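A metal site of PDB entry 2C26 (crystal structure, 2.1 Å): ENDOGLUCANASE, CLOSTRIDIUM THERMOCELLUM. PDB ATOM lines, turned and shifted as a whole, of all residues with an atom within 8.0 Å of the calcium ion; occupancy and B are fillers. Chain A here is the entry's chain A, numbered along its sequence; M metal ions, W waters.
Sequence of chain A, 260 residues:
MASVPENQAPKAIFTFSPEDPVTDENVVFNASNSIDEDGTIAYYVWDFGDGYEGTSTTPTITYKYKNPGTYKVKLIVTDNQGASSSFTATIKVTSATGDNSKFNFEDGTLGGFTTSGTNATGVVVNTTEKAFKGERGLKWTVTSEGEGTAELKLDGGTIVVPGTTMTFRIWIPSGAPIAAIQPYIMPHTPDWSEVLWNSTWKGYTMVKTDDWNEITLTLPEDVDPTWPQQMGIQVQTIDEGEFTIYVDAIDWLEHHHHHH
The side-chain carboxylate (OD1) of Asp 79 is in hydrogen-bond range of the backbone NH (N) of Gln 81 (2.8 Å). The side-chain carboxylate (OD1) of Asp 79 sits at hydrogen-bond distance from the backbone NH (N) of Ala 83 (2.9 Å). OD1 of Asp 79 sits at hydrogen-bond distance from N of Gly 82, 3.0 Å away. N of Gly 39 sits close to OD2 of Asp 36 (3.2 Å). The side-chain carboxylate (OD2) of Asp 36 lies close to the side-chain amide oxygen (OD1) of Asn 80 (3.5 Å). The backbone NH (N) of Thr 40 lies close to the side-chain carboxylate (OD2) of Asp 36 (3.4 Å). The side-chain amide oxygen (OD1) of Asn 7 lies close to the side-chain amide nitrogen (NE2) of Gln 81 (3.0 Å).
Of the 20 residues printed, 5 come within 4 Å of the calcium ion.
The calcium ion is bound by the backbone carbonyl oxygen (O) of Gln 8 (2.4 Å), the side-chain carboxylate (OD1) of Asp 38 (2.4 Å), the side-chain carboxylate (OD2) of Asp 79 (2.4 Å), the side-chain carboxylate (OD1) of Asp 36 (2.4 Å), the side-chain amide oxygen (OD1) of Asn 7 (2.5 Å), the side-chain carboxylate (OD2) of Asp 36 (2.5 Å) and water W1 (2.6 Å). The calcium ion has seven donor atoms within binding distance.
Water W1 bridges the side-chain amide nitrogen of Gln 81 (2.5 Å) and the side-chain amide oxygen of Asn 80 (2.8 Å).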
ATOM      1  N   GLU A   6     -25.315   8.935  13.331  1.00  0.00           N
ATOM      2  CA  GLU A   6     -25.044  10.364  13.074  1.00  0.00           C
ATOM      3  C   GLU A   6     -25.324  11.321  14.242  1.00  0.00           C
ATOM      4  O   GLU A   6     -24.461  12.145  14.560  1.00  0.00           O
ATOM      5  CB  GLU A   6     -25.748  10.833  11.791  1.00  0.00           C
ATOM      6  CG  GLU A   6     -25.342  12.219  11.322  1.00  0.00           C
ATOM      7  CD  GLU A   6     -25.296  12.355   9.796  1.00  0.00           C
ATOM      8  OE1 GLU A   6     -25.289  11.308   9.103  1.00  0.00           O
ATOM      9  OE2 GLU A   6     -25.269  13.509   9.304  1.00  0.00           O
ATOM     10  N   ASN A   7     -26.530  11.259  14.844  1.00  0.00           N
ATOM     11  CA  ASN A   7     -26.774  12.066  16.037  1.00  0.00           C
ATOM     12  C   ASN A   7     -25.880  11.577  17.165  1.00  0.00           C
ATOM     13  O   ASN A   7     -25.739  10.376  17.394  1.00  0.00           O
ATOM     14  CB  ASN A   7     -28.240  12.037  16.486  1.00  0.00           C
ATOM     15  CG  ASN A   7     -28.489  12.814  17.796  1.00  0.00           C
ATOM     16  OD1 ASN A   7     -27.910  13.867  18.034  1.00  0.00           O
ATOM     17  ND2 ASN A   7     -29.382  12.285  18.636  1.00  0.00           N
ATOM     18  N   GLN A   8     -25.269  12.521  17.863  1.00  0.00           N
ATOM     19  CA  GLN A   8     -24.440  12.215  19.009  1.00  0.00           C
ATOM     20  C   GLN A   8     -25.279  12.306  20.260  1.00  0.00           C
ATOM     21  O   GLN A   8     -26.022  13.263  20.457  1.00  0.00           O
ATOM     22  CB  GLN A   8     -23.254  13.178  19.056  1.00  0.00           C
ATOM     23  CG  GLN A   8     -22.162  12.804  20.069  1.00  0.00           C
ATOM     24  CD  GLN A   8     -20.995  13.789  20.026  1.00  0.00           C
ATOM     25  OE1 GLN A   8     -20.511  14.240  21.076  1.00  0.00           O
ATOM     26  NE2 GLN A   8     -20.559  14.127  18.842  1.00  0.00           N
ATOM     27  N   ALA A   9     -25.177  11.294  21.121  1.00  0.00           N
ATOM     28  CA  ALA A   9     -25.903  11.287  22.398  1.00  0.00           C
ATOM     29  C   ALA A   9     -25.328  12.353  23.337  1.00  0.00           C
ATOM     30  O   ALA A   9     -24.138  12.701  23.234  1.00  0.00           O
ATOM     31  CB  ALA A   9     -25.864   9.892  23.030  1.00  0.00           C
ATOM     32  N   PRO A  10     -26.177  12.923  24.219  1.00  0.00           N
ATOM     33  CA  PRO A  10     -25.719  13.948  25.162  1.00  0.00           C
ATOM     34  C   PRO A  10     -24.802  13.455  26.292  1.00  0.00           C
ATOM     35  O   PRO A  10     -24.796  12.265  26.624  1.00  0.00           O
ATOM     36  CB  PRO A  10     -27.029  14.478  25.751  1.00  0.00           C
ATOM     37  CG  PRO A  10     -27.993  13.301  25.625  1.00  0.00           C
ATOM     38  CD  PRO A  10     -27.628  12.671  24.328  1.00  0.00           C
ATOM     39  N   LYS A  11     -24.033  14.385  26.863  1.00  0.00           N
ATOM     40  CA  LYS A  11     -23.273  14.177  28.086  1.00  0.00           C
ATOM     41  C   LYS A  11     -24.232  14.371  29.266  1.00  0.00           C
ATOM     42  O   LYS A  11     -24.850  15.426  29.380  1.00  0.00           O
ATOM     43  CB  LYS A  11     -22.115  15.197  28.155  1.00  0.00           C
ATOM     44  CG  LYS A  11     -21.319  15.147  29.465  1.00  0.00           C
ATOM     45  CD  LYS A  11     -20.483  16.412  29.727  1.00  0.00           C
ATOM     46  CE  LYS A  11     -19.324  16.549  28.766  1.00  0.00           C
ATOM     47  NZ  LYS A  11     -18.539  17.785  29.040  1.00  0.00           N
ATOM     48  N   ILE A  35     -24.605  18.353  28.676  1.00  0.00           N
ATOM     49  CA  ILE A  35     -24.593  19.084  27.404  1.00  0.00           C
ATOM     50  C   ILE A  35     -24.828  18.118  26.243  1.00  0.00           C
ATOM     51  O   ILE A  35     -24.357  16.977  26.255  1.00  0.00           O
ATOM     52  CB  ILE A  35     -23.270  19.901  27.198  1.00  0.00           C
ATOM     53  CG1 ILE A  35     -23.232  20.600  25.827  1.00  0.00           C
ATOM     54  CG2 ILE A  35     -21.993  19.032  27.427  1.00  0.00           C
ATOM     55  CD1 ILE A  35     -22.281  21.837  25.767  1.00  0.00           C
ATOM     56  N   ASP A  36     -25.568  18.586  25.249  1.00  0.00           N
ATOM     57  CA  ASP A  36     -25.614  17.900  23.976  1.00  0.00           C
ATOM     58  C   ASP A  36     -24.704  18.661  23.012  1.00  0.00           C
ATOM     59  O   ASP A  36     -24.938  19.834  22.724  1.00  0.00           O
ATOM     60  CB  ASP A  36     -27.045  17.846  23.432  1.00  0.00           C
ATOM     61  CG  ASP A  36     -27.151  16.954  22.216  1.00  0.00           C
ATOM     62  OD1 ASP A  36     -26.467  15.911  22.191  1.00  0.00           O
ATOM     63  OD2 ASP A  36     -27.901  17.270  21.271  1.00  0.00           O
ATOM     64  N   GLU A  37     -23.640  17.996  22.546  1.00  0.00           N
ATOM     65  CA  GLU A  37     -22.583  18.659  21.767  1.00  0.00           C
ATOM     66  C   GLU A  37     -23.038  19.150  20.380  1.00  0.00           C
ATOM     67  O   GLU A  37     -22.500  20.124  19.867  1.00  0.00           O
ATOM     68  CB  GLU A  37     -21.356  17.758  21.610  1.00  0.00           C
ATOM     69  CG  GLU A  37     -20.762  17.210  22.916  1.00  0.00           C
ATOM     70  CD  GLU A  37     -20.161  18.284  23.804  1.00  0.00           C
ATOM     71  OE1 GLU A  37     -19.929  19.425  23.347  1.00  0.00           O
ATOM     72  OE2 GLU A  37     -19.888  17.977  24.988  1.00  0.00           O
ATOM     73  N   ASP A  38     -24.000  18.444  19.788  1.00  0.00           N
ATOM     74  CA  ASP A  38     -24.458  18.737  18.425  1.00  0.00           C
ATOM     75  C   ASP A  38     -25.951  19.098  18.354  1.00  0.00           C
ATOM     76  O   ASP A  38     -26.565  19.005  17.293  1.00  0.00           O
ATOM     77  CB  ASP A  38     -24.163  17.532  17.520  1.00  0.00           C
ATOM     78  CG  ASP A  38     -24.981  16.319  17.900  1.00  0.00           C
ATOM     79  OD1 ASP A  38     -25.525  16.311  19.011  1.00  0.00           O
ATOM     80  OD2 ASP A  38     -25.098  15.390  17.087  1.00  0.00           O
ATOM     81  N   GLY A  39     -26.543  19.486  19.480  1.00  0.00           N
ATOM     82  CA  GLY A  39     -27.962  19.839  19.536  1.00  0.00           C
ATOM     83  C   GLY A  39     -28.281  20.503  20.857  1.00  0.00           C
ATOM     84  O   GLY A  39     -27.457  21.237  21.398  1.00  0.00           O
ATOM     85  N   THR A  40     -29.468  20.241  21.402  1.00  0.00           N
ATOM     86  CA  THR A  40     -29.852  20.788  22.698  1.00  0.00           C
ATOM     87  C   THR A  40     -30.436  19.701  23.596  1.00  0.00           C
ATOM     88  O   THR A  40     -30.880  18.655  23.108  1.00  0.00           O
ATOM     89  CB  THR A  40     -30.900  21.917  22.576  1.00  0.00           C
ATOM     90  OG1 THR A  40     -32.077  21.423  21.920  1.00  0.00           O
ATOM     91  CG2 THR A  40     -30.348  23.122  21.825  1.00  0.00           C
ATOM     92  N   ILE A  41     -30.464  19.962  24.891  1.00  0.00           N
ATOM     93  CA  ILE A  41     -31.130  19.048  25.829  1.00  0.00           C
ATOM     94  C   ILE A  41     -32.612  19.348  25.887  1.00  0.00           C
ATOM     95  O   ILE A  41     -33.021  20.488  26.099  1.00  0.00           O
ATOM     96  CB  ILE A  41     -30.506  19.085  27.252  1.00  0.00           C
ATOM     97  CG1 ILE A  41     -29.034  18.641  27.183  1.00  0.00           C
ATOM     98  CG2 ILE A  41     -31.336  18.215  28.253  1.00  0.00           C
ATOM     99  CD1 ILE A  41     -28.279  18.828  28.469  1.00  0.00           C
ATOM    100  N   THR A  78     -31.979  13.666  27.770  1.00  0.00           N
ATOM    101  CA  THR A  78     -32.436  13.324  26.428  1.00  0.00           C
ATOM    102  C   THR A  78     -32.313  14.554  25.536  1.00  0.00           C
ATOM    103  O   THR A  78     -32.748  15.636  25.920  1.00  0.00           O
ATOM    104  CB  THR A  78     -33.912  12.813  26.451  1.00  0.00           C
ATOM    105  OG1 THR A  78     -34.021  11.689  27.340  1.00  0.00           O
ATOM    106  CG2 THR A  78     -34.376  12.386  25.055  1.00  0.00           C
ATOM    107  N   ASP A  79     -31.707  14.394  24.359  1.00  0.00           N
ATOM    108  CA  ASP A  79     -31.501  15.525  23.475  1.00  0.00           C
ATOM    109  C   ASP A  79     -32.712  15.789  22.568  1.00  0.00           C
ATOM    110  O   ASP A  79     -33.733  15.090  22.661  1.00  0.00           O
ATOM    111  CB  ASP A  79     -30.178  15.387  22.670  1.00  0.00           C
ATOM    112  CG  ASP A  79     -30.216  14.271  21.612  1.00  0.00           C
ATOM    113  OD1 ASP A  79     -31.284  13.779  21.237  1.00  0.00           O
ATOM    114  OD2 ASP A  79     -29.136  13.869  21.155  1.00  0.00           O
ATOM    115  N   ASN A  80     -32.595  16.803  21.707  1.00  0.00           N
ATOM    116  CA  ASN A  80     -33.683  17.203  20.789  1.00  0.00           C
ATOM    117  C   ASN A  80     -34.041  16.148  19.732  1.00  0.00           C
ATOM    118  O   ASN A  80     -35.015  16.309  19.010  1.00  0.00           O
ATOM    119  CB  ASN A  80     -33.317  18.529  20.090  1.00  0.00           C
ATOM    120  CG  ASN A  80     -32.043  18.420  19.280  1.00  0.00           C
ATOM    121  OD1 ASN A  80     -30.949  18.201  19.826  1.00  0.00           O
ATOM    122  ND2 ASN A  80     -32.170  18.560  17.961  1.00  0.00           N
ATOM    123  N   GLN A  81     -33.239  15.085  19.627  1.00  0.00           N
ATOM    124  CA  GLN A  81     -33.526  14.020  18.663  1.00  0.00           C
ATOM    125  C   GLN A  81     -33.856  12.683  19.323  1.00  0.00           C
ATOM    126  O   GLN A  81     -33.978  11.660  18.657  1.00  0.00           O
ATOM    127  CB  GLN A  81     -32.389  13.877  17.643  1.00  0.00           C
ATOM    128  CG  GLN A  81     -32.314  15.032  16.622  1.00  0.00           C
ATOM    129  CD  GLN A  81     -31.032  14.994  15.799  1.00  0.00           C
ATOM    130  OE1 GLN A  81     -31.044  14.595  14.635  1.00  0.00           O
ATOM    131  NE2 GLN A  81     -29.930  15.405  16.403  1.00  0.00           N
ATOM    132  N   GLY A  82     -34.033  12.712  20.648  1.00  0.00           N
ATOM    133  CA  GLY A  82     -34.488  11.529  21.365  1.00  0.00           C
ATOM    134  C   GLY A  82     -33.382  10.608  21.852  1.00  0.00           C
ATOM    135  O   GLY A  82     -33.677   9.553  22.411  1.00  0.00           O
ATOM    136  N   ALA A  83     -32.123  10.989  21.644  1.00  0.00           N
ATOM    137  CA  ALA A  83     -30.974  10.222  22.156  1.00  0.00           C
ATOM    138  C   ALA A  83     -30.724  10.558  23.634  1.00  0.00           C
ATOM    139  O   ALA A  83     -30.833  11.729  24.040  1.00  0.00           O
ATOM    140  CB  ALA A  83     -29.723  10.460  21.327  1.00  0.00           C
ATOM    141  N   SER A  84     -30.411   9.546  24.429  1.00  0.00           N
ATOM    142  CA  SER A  84     -30.239   9.756  25.856  1.00  0.00           C
ATOM    143  C   SER A  84     -28.958   9.122  26.435  1.00  0.00           C
ATOM    144  O   SER A  84     -28.421   8.157  25.869  1.00  0.00           O
ATOM    145  CB  SER A  84     -31.454   9.232  26.608  1.00  0.00           C
ATOM    146  OG  SER A  84     -31.581   7.842  26.368  1.00  0.00           O
HETATM  147 CA    CA M   1     -27.395  15.179  20.045  1.00  0.00          CA
HETATM  148  O   HOH W   1     -29.358  16.208  18.754  1.00  0.00           O
